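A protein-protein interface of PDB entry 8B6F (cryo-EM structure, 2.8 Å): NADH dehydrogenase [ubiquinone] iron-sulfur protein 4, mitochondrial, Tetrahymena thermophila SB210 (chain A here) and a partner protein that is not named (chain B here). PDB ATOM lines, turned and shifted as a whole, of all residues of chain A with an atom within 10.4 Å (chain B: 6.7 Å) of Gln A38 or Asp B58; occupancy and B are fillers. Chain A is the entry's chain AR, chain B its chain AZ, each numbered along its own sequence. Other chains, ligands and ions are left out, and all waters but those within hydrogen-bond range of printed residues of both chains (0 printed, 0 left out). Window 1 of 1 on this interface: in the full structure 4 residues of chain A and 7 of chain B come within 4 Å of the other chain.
The backbone NH of Asp B58 is in hydrogen-bond range of the side-chain amide oxygen of Gln A38. OD1 of Asp B58 is in hydrogen-bond range of ND2 of Asn A41 (3.0 Å). The backbone carbonyl oxygen (O) of Asn A41 sits close to the backbone carbonyl oxygen (O) of Glu B56, at 3.5 Å.
The backbone carbonyl oxygen (O) of Ala A37 is in hydrogen-bond range of the side-chain amide nitrogen (ND2) of Asn A41 (2.9 Å). O of Asn A41 is in hydrogen-bond range of NZ of Lys A45, 3.3 Å away. N of Tyr B60 sits at hydrogen-bond distance from O of Val B18 (2.8 Å). O of Phe B19 sits at hydrogen-bond distance from N of Cys B54 (2.9 Å). The side-chain sulfur of Cys B20 sits at hydrogen-bond distance from the backbone NH of Glu B56, at 3.3 Å. The side-chain carboxylate (OD1) of Asp B58 lies within salt-bridge range of the guanidinium group (NH2) of Arg B25 (2.8 Å).
Tyr B60 touches Val A34. Ala B57 touches Gln A38 (CA to OE1, 3.8 Å). CD2 of Tyr B60 touches NE2 of Gln A38, 3.4 Å away. CD1 of Ile A42 touches SG of Cys B54, 3.6 Å away. Glu B55 touches Ile A42 (O to CG1, 3.8 Å).
Ala A24 touches none of the printed residues of chain B. Printed residues of chain B within 4 Å of Val A34: Tyr B60 (3.9 Å). Gln A38 touches just these residues of chain B: Ala B57 (3.8 Å), Asp B58 (3.2 Å) and Tyr B60 (3.4 Å). Printed residues of chain B within 4 Å of Ile A42: Cys B54 and Glu B55. No residue of chain A comes within 4 Å of Val B18. Printed residues of chain A within 4 Å of Cys B54: Ile A42. Of the printed residues of chain A, Glu B55 touches Ile A42 (3.8 Å). Of the printed residues of chain A, Glu B56 touches Asn A41. Ala B57 touches one residue of chain A. No residue of chain A comes within 4 Å of Pro B59. Tyr B60 touches just these residues of chain A: Val A34 and Gln A38. Phe B74 touches none of the printed residues of chain A. The nearest printed residue of chain A that does not touch Glu B56 is Ile A42 (4.1 Å).
Of the 16 printed residues of chain B, 6 touch a printed residue of chain A. Printed residues of chain B that touch a printed residue of chain A: Cys B54, Glu B55, Glu B56, Ala B57, Asp B58 and Tyr B60. Hydrophobic or aromatic side chains of chain B that line the printed part of chain A: Ala B57 and Tyr B60. Of the 18 printed residues of chain A, 4 touch a printed residue of chain B. Printed residues of chain A that touch a printed residue of chain B: Val A34, Gln A38, Asn A41 and Ile A42. Hydrophobic or aromatic side chains of chain A that line the printed part of chain B: Val A34 and Ile A42. Among the printed residues, no Asp or Glu carboxylate lies within 4 Å of a Lys or Arg side-chain nitrogen of the other chain.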
ATOM      1  N   ALA A  21      -2.157  16.729 -26.501  1.00  0.00           N
ATOM      2  CA  ALA A  21      -2.401  16.563 -25.075  1.00  0.00           C
ATOM      3  C   ALA A  21      -3.551  15.585 -24.884  1.00  0.00           C
ATOM      4  O   ALA A  21      -4.590  15.707 -25.540  1.00  0.00           O
ATOM      5  CB  ALA A  21      -2.726  17.905 -24.418  1.00  0.00           C
ATOM      6  N   LYS A  22      -3.363  14.616 -23.992  1.00  0.00           N
ATOM      7  CA  LYS A  22      -4.345  13.554 -23.838  1.00  0.00           C
ATOM      8  C   LYS A  22      -5.639  14.083 -23.232  1.00  0.00           C
ATOM      9  O   LYS A  22      -5.649  15.051 -22.468  1.00  0.00           O
ATOM     10  CB  LYS A  22      -3.799  12.422 -22.971  1.00  0.00           C
ATOM     11  CG  LYS A  22      -4.660  11.165 -23.040  1.00  0.00           C
ATOM     12  CD  LYS A  22      -4.104  10.065 -22.175  1.00  0.00           C
ATOM     13  CE  LYS A  22      -4.906   8.786 -22.283  1.00  0.00           C
ATOM     14  NZ  LYS A  22      -4.878   8.229 -23.660  1.00  0.00           N
ATOM     15  N   ALA A  24      -8.820  12.612 -21.005  1.00  0.00           N
ATOM     16  CA  ALA A  24      -9.215  11.474 -20.186  1.00  0.00           C
ATOM     17  C   ALA A  24     -10.504  10.865 -20.717  1.00  0.00           C
ATOM     18  O   ALA A  24     -11.545  11.528 -20.759  1.00  0.00           O
ATOM     19  CB  ALA A  24      -9.391  11.911 -18.733  1.00  0.00           C
ATOM     20  N   GLU A  29      -8.566   6.821 -16.312  1.00  0.00           N
ATOM     21  CA  GLU A  29      -8.026   8.129 -16.669  1.00  0.00           C
ATOM     22  C   GLU A  29      -8.835   9.249 -16.029  1.00  0.00           C
ATOM     23  O   GLU A  29      -8.267  10.234 -15.543  1.00  0.00           O
ATOM     24  CB  GLU A  29      -7.995   8.281 -18.189  1.00  0.00           C
ATOM     25  CG  GLU A  29      -7.136   7.232 -18.881  1.00  0.00           C
ATOM     26  CD  GLU A  29      -7.199   7.328 -20.393  1.00  0.00           C
ATOM     27  OE1 GLU A  29      -7.965   8.167 -20.907  1.00  0.00           O
ATOM     28  OE2 GLU A  29      -6.476   6.565 -21.067  1.00  0.00           O
ATOM     29  N   LEU A  32      -7.890   9.519 -12.505  1.00  0.00           N
ATOM     30  CA  LEU A  32      -6.577  10.149 -12.438  1.00  0.00           C
ATOM     31  C   LEU A  32      -6.509  11.438 -13.247  1.00  0.00           C
ATOM     32  O   LEU A  32      -5.429  11.816 -13.718  1.00  0.00           O
ATOM     33  CB  LEU A  32      -5.510   9.165 -12.918  1.00  0.00           C
ATOM     34  CG  LEU A  32      -5.514   7.803 -12.220  1.00  0.00           C
ATOM     35  CD1 LEU A  32      -4.566   6.838 -12.910  1.00  0.00           C
ATOM     36  CD2 LEU A  32      -5.151   7.953 -10.754  1.00  0.00           C
ATOM     37  N   SER A  33      -7.645  12.118 -13.428  1.00  0.00           N
ATOM     38  CA  SER A  33      -7.682  13.314 -14.264  1.00  0.00           C
ATOM     39  C   SER A  33      -6.603  14.314 -13.869  1.00  0.00           C
ATOM     40  O   SER A  33      -5.979  14.938 -14.734  1.00  0.00           O
ATOM     41  CB  SER A  33      -9.064  13.963 -14.183  1.00  0.00           C
ATOM     42  OG  SER A  33      -9.389  14.312 -12.849  1.00  0.00           O
ATOM     43  N   VAL A  34      -6.374  14.491 -12.567  1.00  0.00           N
ATOM     44  CA  VAL A  34      -5.336  15.420 -12.129  1.00  0.00           C
ATOM     45  C   VAL A  34      -3.982  14.987 -12.671  1.00  0.00           C
ATOM     46  O   VAL A  34      -3.163  15.820 -13.079  1.00  0.00           O
ATOM     47  CB  VAL A  34      -5.325  15.529 -10.592  1.00  0.00           C
ATOM     48  CG1 VAL A  34      -4.174  16.408 -10.119  1.00  0.00           C
ATOM     49  CG2 VAL A  34      -6.651  16.076 -10.091  1.00  0.00           C
ATOM     50  N   GLY A  35      -3.722  13.679 -12.684  1.00  0.00           N
ATOM     51  CA  GLY A  35      -2.473  13.192 -13.243  1.00  0.00           C
ATOM     52  C   GLY A  35      -2.343  13.493 -14.723  1.00  0.00           C
ATOM     53  O   GLY A  35      -1.269  13.867 -15.199  1.00  0.00           O
ATOM     54  N   VAL A  36      -3.435  13.331 -15.472  1.00  0.00           N
ATOM     55  CA  VAL A  36      -3.407  13.639 -16.899  1.00  0.00           C
ATOM     56  C   VAL A  36      -3.122  15.118 -17.114  1.00  0.00           C
ATOM     57  O   VAL A  36      -2.329  15.494 -17.985  1.00  0.00           O
ATOM     58  CB  VAL A  36      -4.727  13.209 -17.565  1.00  0.00           C
ATOM     59  CG1 VAL A  36      -4.732  13.585 -19.040  1.00  0.00           C
ATOM     60  CG2 VAL A  36      -4.944  11.714 -17.397  1.00  0.00           C
ATOM     61  N   ALA A  37      -3.765  15.981 -16.325  1.00  0.00           N
ATOM     62  CA  ALA A  37      -3.521  17.414 -16.453  1.00  0.00           C
ATOM     63  C   ALA A  37      -2.072  17.757 -16.134  1.00  0.00           C
ATOM     64  O   ALA A  37      -1.450  18.562 -16.836  1.00  0.00           O
ATOM     65  CB  ALA A  37      -4.469  18.189 -15.538  1.00  0.00           C
ATOM     66  N   GLN A  38      -1.519  17.161 -15.076  1.00  0.00           N
ATOM     67  CA  GLN A  38      -0.125  17.421 -14.734  1.00  0.00           C
ATOM     68  C   GLN A  38       0.806  16.958 -15.845  1.00  0.00           C
ATOM     69  O   GLN A  38       1.751  17.666 -16.210  1.00  0.00           O
ATOM     70  CB  GLN A  38       0.232  16.733 -13.417  1.00  0.00           C
ATOM     71  CG  GLN A  38      -0.488  17.289 -12.197  1.00  0.00           C
ATOM     72  CD  GLN A  38       0.054  18.636 -11.756  1.00  0.00           C
ATOM     73  OE1 GLN A  38       0.575  19.405 -12.561  1.00  0.00           O
ATOM     74  NE2 GLN A  38      -0.060  18.922 -10.465  1.00  0.00           N
ATOM     75  N   LYS A  39       0.554  15.771 -16.400  1.00  0.00           N
ATOM     76  CA  LYS A  39       1.391  15.267 -17.483  1.00  0.00           C
ATOM     77  C   LYS A  39       1.329  16.188 -18.696  1.00  0.00           C
ATOM     78  O   LYS A  39       2.358  16.485 -19.312  1.00  0.00           O
ATOM     79  CB  LYS A  39       0.961  13.848 -17.855  1.00  0.00           C
ATOM     80  CG  LYS A  39       1.896  13.145 -18.828  1.00  0.00           C
ATOM     81  CD  LYS A  39       1.264  12.995 -20.202  1.00  0.00           C
ATOM     82  CE  LYS A  39       2.148  12.177 -21.132  1.00  0.00           C
ATOM     83  NZ  LYS A  39       2.342  10.783 -20.648  1.00  0.00           N
ATOM     84  N   ASN A  40       0.131  16.655 -19.049  1.00  0.00           N
ATOM     85  CA  ASN A  40      -0.004  17.574 -20.175  1.00  0.00           C
ATOM     86  C   ASN A  40       0.739  18.878 -19.918  1.00  0.00           C
ATOM     87  O   ASN A  40       1.395  19.416 -20.817  1.00  0.00           O
ATOM     88  CB  ASN A  40      -1.481  17.855 -20.453  1.00  0.00           C
ATOM     89  CG  ASN A  40      -2.233  16.624 -20.906  1.00  0.00           C
ATOM     90  OD1 ASN A  40      -1.641  15.673 -21.412  1.00  0.00           O
ATOM     91  ND2 ASN A  40      -3.549  16.638 -20.736  1.00  0.00           N
ATOM     92  N   ASN A  41       0.649  19.404 -18.695  1.00  0.00           N
ATOM     93  CA  ASN A  41       1.304  20.670 -18.384  1.00  0.00           C
ATOM     94  C   ASN A  41       2.821  20.542 -18.374  1.00  0.00           C
ATOM     95  O   ASN A  41       3.522  21.510 -18.689  1.00  0.00           O
ATOM     96  CB  ASN A  41       0.822  21.190 -17.030  1.00  0.00           C
ATOM     97  CG  ASN A  41      -0.663  21.474 -17.010  1.00  0.00           C
ATOM     98  OD1 ASN A  41      -1.255  21.821 -18.031  1.00  0.00           O
ATOM     99  ND2 ASN A  41      -1.276  21.331 -15.840  1.00  0.00           N
ATOM    100  N   ILE A  42       3.344  19.374 -18.020  1.00  0.00           N
ATOM    101  CA  ILE A  42       4.777  19.222 -17.790  1.00  0.00           C
ATOM    102  C   ILE A  42       5.511  18.731 -19.031  1.00  0.00           C
ATOM    103  O   ILE A  42       6.643  19.147 -19.289  1.00  0.00           O
ATOM    104  CB  ILE A  42       4.986  18.279 -16.591  1.00  0.00           C
ATOM    105  CG1 ILE A  42       4.594  19.001 -15.305  1.00  0.00           C
ATOM    106  CG2 ILE A  42       6.432  17.802 -16.508  1.00  0.00           C
ATOM    107  CD1 ILE A  42       4.261  18.077 -14.184  1.00  0.00           C
ATOM    108  N   GLN A  43       4.906  17.846 -19.818  1.00  0.00           N
ATOM    109  CA  GLN A  43       5.619  17.274 -20.947  1.00  0.00           C
ATOM    110  C   GLN A  43       5.979  18.371 -21.950  1.00  0.00           C
ATOM    111  O   GLN A  43       5.278  19.381 -22.054  1.00  0.00           O
ATOM    112  CB  GLN A  43       4.780  16.192 -21.623  1.00  0.00           C
ATOM    113  CG  GLN A  43       3.514  16.700 -22.287  1.00  0.00           C
ATOM    114  CD  GLN A  43       2.717  15.583 -22.929  1.00  0.00           C
ATOM    115  OE1 GLN A  43       3.118  14.421 -22.890  1.00  0.00           O
ATOM    116  NE2 GLN A  43       1.583  15.929 -23.524  1.00  0.00           N
ATOM    117  N   PRO A  44       7.073  18.203 -22.694  1.00  0.00           N
ATOM    118  CA  PRO A  44       7.470  19.240 -23.656  1.00  0.00           C
ATOM    119  C   PRO A  44       6.381  19.485 -24.689  1.00  0.00           C
ATOM    120  O   PRO A  44       5.707  18.559 -25.139  1.00  0.00           O
ATOM    121  CB  PRO A  44       8.741  18.667 -24.295  1.00  0.00           C
ATOM    122  CG  PRO A  44       8.671  17.200 -24.050  1.00  0.00           C
ATOM    123  CD  PRO A  44       7.973  17.039 -22.738  1.00  0.00           C
ATOM    124  N   LYS A  45       6.224  20.750 -25.076  1.00  0.00           N
ATOM    125  CA  LYS A  45       5.142  21.110 -25.986  1.00  0.00           C
ATOM    126  C   LYS A  45       5.410  20.635 -27.409  1.00  0.00           C
ATOM    127  O   LYS A  45       4.469  20.262 -28.120  1.00  0.00           O
ATOM    128  CB  LYS A  45       4.924  22.623 -25.962  1.00  0.00           C
ATOM    129  CG  LYS A  45       4.735  23.201 -24.561  1.00  0.00           C
ATOM    130  CD  LYS A  45       3.527  22.590 -23.859  1.00  0.00           C
ATOM    131  CE  LYS A  45       3.360  23.144 -22.453  1.00  0.00           C
ATOM    132  NZ  LYS A  45       4.506  22.796 -21.566  1.00  0.00           N
ATOM    133  N   VAL B  18       2.518  19.833  -4.326  1.00  0.00           N
ATOM    134  CA  VAL B  18       3.089  19.688  -5.659  1.00  0.00           C
ATOM    135  C   VAL B  18       2.877  21.002  -6.398  1.00  0.00           C
ATOM    136  O   VAL B  18       1.733  21.423  -6.605  1.00  0.00           O
ATOM    137  CB  VAL B  18       2.456  18.514  -6.420  1.00  0.00           C
ATOM    138  CG1 VAL B  18       3.074  18.372  -7.803  1.00  0.00           C
ATOM    139  CG2 VAL B  18       2.603  17.224  -5.628  1.00  0.00           C
ATOM    140  N   PHE B  19       3.965  21.652  -6.800  1.00  0.00           N
ATOM    141  CA  PHE B  19       3.855  22.967  -7.419  1.00  0.00           C
ATOM    142  C   PHE B  19       5.087  23.219  -8.280  1.00  0.00           C
ATOM    143  O   PHE B  19       5.970  22.367  -8.406  1.00  0.00           O
ATOM    144  CB  PHE B  19       3.681  24.054  -6.356  1.00  0.00           C
ATOM    145  CG  PHE B  19       4.827  24.152  -5.395  1.00  0.00           C
ATOM    146  CD1 PHE B  19       4.931  23.276  -4.329  1.00  0.00           C
ATOM    147  CD2 PHE B  19       5.796  25.128  -5.551  1.00  0.00           C
ATOM    148  CE1 PHE B  19       5.982  23.366  -3.441  1.00  0.00           C
ATOM    149  CE2 PHE B  19       6.852  25.222  -4.668  1.00  0.00           C
ATOM    150  CZ  PHE B  19       6.945  24.340  -3.610  1.00  0.00           C
ATOM    151  N   CYS B  20       5.132  24.407  -8.878  1.00  0.00           N
ATOM    152  CA  CYS B  20       6.247  24.856  -9.696  1.00  0.00           C
ATOM    153  C   CYS B  20       7.102  25.852  -8.923  1.00  0.00           C
ATOM    154  O   CYS B  20       6.598  26.620  -8.099  1.00  0.00           O
ATOM    155  CB  CYS B  20       5.750  25.499 -10.991  1.00  0.00           C
ATOM    156  SG  CYS B  20       7.050  26.274 -11.973  1.00  0.00           S
ATOM    157  N   ARG B  25       1.809  31.475 -10.835  1.00  0.00           N
ATOM    158  CA  ARG B  25       0.632  30.700 -10.464  1.00  0.00           C
ATOM    159  C   ARG B  25       0.867  29.906  -9.185  1.00  0.00           C
ATOM    160  O   ARG B  25      -0.088  29.594  -8.465  1.00  0.00           O
ATOM    161  CB  ARG B  25       0.249  29.768 -11.613  1.00  0.00           C
ATOM    162  CG  ARG B  25      -1.047  29.010 -11.395  1.00  0.00           C
ATOM    163  CD  ARG B  25      -1.419  28.188 -12.619  1.00  0.00           C
ATOM    164  NE  ARG B  25      -0.349  27.274 -13.004  1.00  0.00           N
ATOM    165  CZ  ARG B  25      -0.411  26.434 -14.027  1.00  0.00           C
ATOM    166  NH1 ARG B  25      -1.486  26.355 -14.794  1.00  0.00           N
ATOM    167  NH2 ARG B  25       0.633  25.654 -14.291  1.00  0.00           N
ATOM    168  N   SER B  26       2.121  29.569  -8.888  1.00  0.00           N
ATOM    169  CA  SER B  26       2.475  28.833  -7.683  1.00  0.00           C
ATOM    170  C   SER B  26       3.114  29.710  -6.615  1.00  0.00           C
ATOM    171  O   SER B  26       3.244  29.264  -5.470  1.00  0.00           O
ATOM    172  CB  SER B  26       3.431  27.685  -8.027  1.00  0.00           C
ATOM    173  OG  SER B  26       4.648  28.178  -8.560  1.00  0.00           O
ATOM    174  N   LEU B  29       1.763  29.489  -2.914  1.00  0.00           N
ATOM    175  CA  LEU B  29       2.013  28.237  -2.208  1.00  0.00           C
ATOM    176  C   LEU B  29       3.502  28.041  -1.962  1.00  0.00           C
ATOM    177  O   LEU B  29       3.909  27.560  -0.898  1.00  0.00           O
ATOM    178  CB  LEU B  29       1.436  27.067  -3.005  1.00  0.00           C
ATOM    179  CG  LEU B  29       1.673  25.667  -2.434  1.00  0.00           C
ATOM    180  CD1 LEU B  29       1.076  25.534  -1.043  1.00  0.00           C
ATOM    181  CD2 LEU B  29       1.093  24.622  -3.365  1.00  0.00           C
ATOM    182  N   CYS B  54       8.040  20.875  -9.766  1.00  0.00           N
ATOM    183  CA  CYS B  54       8.173  20.536 -11.176  1.00  0.00           C
ATOM    184  C   CYS B  54       7.765  21.748 -11.997  1.00  0.00           C
ATOM    185  O   CYS B  54       6.731  22.362 -11.724  1.00  0.00           O
ATOM    186  CB  CYS B  54       7.327  19.315 -11.542  1.00  0.00           C
ATOM    187  SG  CYS B  54       7.706  18.653 -13.176  1.00  0.00           S
ATOM    188  N   GLU B  55       8.576  22.083 -12.996  1.00  0.00           N
ATOM    189  CA  GLU B  55       8.342  23.291 -13.775  1.00  0.00           C
ATOM    190  C   GLU B  55       7.017  23.208 -14.521  1.00  0.00           C
ATOM    191  O   GLU B  55       6.652  22.164 -15.068  1.00  0.00           O
ATOM    192  CB  GLU B  55       9.492  23.507 -14.758  1.00  0.00           C
ATOM    193  CG  GLU B  55       9.417  24.822 -15.514  1.00  0.00           C
ATOM    194  CD  GLU B  55      10.687  25.125 -16.281  1.00  0.00           C
ATOM    195  OE1 GLU B  55      11.679  24.389 -16.103  1.00  0.00           O
ATOM    196  OE2 GLU B  55      10.694  26.100 -17.063  1.00  0.00           O
ATOM    197  N   GLU B  56       6.297  24.331 -14.541  1.00  0.00           N
ATOM    198  CA  GLU B  56       5.010  24.440 -15.228  1.00  0.00           C
ATOM    199  C   GLU B  56       4.016  23.400 -14.714  1.00  0.00           C
ATOM    200  O   GLU B  56       3.248  22.817 -15.480  1.00  0.00           O
ATOM    201  CB  GLU B  56       5.186  24.317 -16.743  1.00  0.00           C
ATOM    202  CG  GLU B  56       5.967  25.460 -17.375  1.00  0.00           C
ATOM    203  CD  GLU B  56       5.243  26.788 -17.279  1.00  0.00           C
ATOM    204  OE1 GLU B  56       4.060  26.796 -16.878  1.00  0.00           O
ATOM    205  OE2 GLU B  56       5.856  27.827 -17.605  1.00  0.00           O
ATOM    206  N   ALA B  57       4.029  23.171 -13.406  1.00  0.00           N
ATOM    207  CA  ALA B  57       3.094  22.271 -12.750  1.00  0.00           C
ATOM    208  C   ALA B  57       2.023  23.071 -12.023  1.00  0.00           C
ATOM    209  O   ALA B  57       2.301  24.133 -11.460  1.00  0.00           O
ATOM    210  CB  ALA B  57       3.818  21.357 -11.760  1.00  0.00           C
ATOM    211  N   ASP B  58       0.796  22.567 -12.054  1.00  0.00           N
ATOM    212  CA  ASP B  58      -0.302  23.229 -11.358  1.00  0.00           C
ATOM    213  C   ASP B  58      -0.129  23.075  -9.851  1.00  0.00           C
ATOM    214  O   ASP B  58       0.145  21.967  -9.376  1.00  0.00           O
ATOM    215  CB  ASP B  58      -1.643  22.642 -11.789  1.00  0.00           C
ATOM    216  CG  ASP B  58      -1.997  22.982 -13.221  1.00  0.00           C
ATOM    217  OD1 ASP B  58      -1.165  23.608 -13.910  1.00  0.00           O
ATOM    218  OD2 ASP B  58      -3.111  22.627 -13.657  1.00  0.00           O
ATOM    219  N   PRO B  59      -0.270  24.144  -9.066  1.00  0.00           N
ATOM    220  CA  PRO B  59      -0.201  23.989  -7.608  1.00  0.00           C
ATOM    221  C   PRO B  59      -1.295  23.060  -7.109  1.00  0.00           C
ATOM    222  O   PRO B  59      -2.430  23.095  -7.584  1.00  0.00           O
ATOM    223  CB  PRO B  59      -0.390  25.416  -7.085  1.00  0.00           C
ATOM    224  CG  PRO B  59      -0.037  26.295  -8.223  1.00  0.00           C
ATOM    225  CD  PRO B  59      -0.442  25.555  -9.455  1.00  0.00           C
ATOM    226  N   TYR B  60      -0.944  22.224  -6.134  1.00  0.00           N
ATOM    227  CA  TYR B  60      -1.890  21.262  -5.586  1.00  0.00           C
ATOM    228  C   TYR B  60      -1.476  20.901  -4.170  1.00  0.00           C
ATOM    229  O   TYR B  60      -0.301  20.622  -3.916  1.00  0.00           O
ATOM    230  CB  TYR B  60      -1.963  20.001  -6.454  1.00  0.00           C
ATOM    231  CG  TYR B  60      -3.009  20.064  -7.541  1.00  0.00           C
ATOM    232  CD1 TYR B  60      -4.338  19.763  -7.270  1.00  0.00           C
ATOM    233  CD2 TYR B  60      -2.668  20.414  -8.839  1.00  0.00           C
ATOM    234  CE1 TYR B  60      -5.298  19.816  -8.262  1.00  0.00           C
ATOM    235  CE2 TYR B  60      -3.620  20.471  -9.837  1.00  0.00           C
ATOM    236  CZ  TYR B  60      -4.934  20.170  -9.543  1.00  0.00           C
ATOM    237  OH  TYR B  60      -5.884  20.225 -10.534  1.00  0.00           O
ATOM    238  N   PHE B  74      -6.850  22.626  -5.462  1.00  0.00           N
ATOM    239  CA  PHE B  74      -6.183  23.433  -6.476  1.00  0.00           C
ATOM    240  C   PHE B  74      -5.885  24.807  -5.885  1.00  0.00           C
ATOM    241  O   PHE B  74      -6.801  25.597  -5.639  1.00  0.00           O
ATOM    242  CB  PHE B  74      -7.070  23.527  -7.714  1.00  0.00           C
ATOM    243  CG  PHE B  74      -6.452  24.273  -8.855  1.00  0.00           C
ATOM    244  CD1 PHE B  74      -5.327  23.783  -9.495  1.00  0.00           C
ATOM    245  CD2 PHE B  74      -7.022  25.448  -9.315  1.00  0.00           C
ATOM    246  CE1 PHE B  74      -4.767  24.464 -10.557  1.00  0.00           C
ATOM    247  CE2 PHE B  74      -6.466  26.135 -10.375  1.00  0.00           C
ATOM    248  CZ  PHE B  74      -5.337  25.641 -10.998  1.00  0.00           C
ATOM    249  N   ALA B  75      -4.604  25.094  -5.659  1.00  0.00           N
ATOM    250  CA  ALA B  75      -4.166  26.284  -4.937  1.00  0.00           C
ATOM    251  C   ALA B  75      -3.465  27.285  -5.851  1.00  0.00           C
ATOM    252  O   ALA B  75      -2.469  27.902  -5.472  1.00  0.00           O
ATOM    253  CB  ALA B  75      -3.247  25.896  -3.782  1.00  0.00           C
ATOM    254  N   ALA B  76      -3.980  27.459  -7.063  1.00  0.00           N
ATOM    255  CA  ALA B  76      -3.384  28.389  -8.011  1.00  0.00           C
ATOM    256  C   ALA B  76      -3.830  29.815  -7.719  1.00  0.00           C
ATOM    257  O   ALA B  76      -5.006  30.072  -7.448  1.00  0.00           O
ATOM    258  CB  ALA B  76      -3.768  28.009  -9.439  1.00  0.00           C
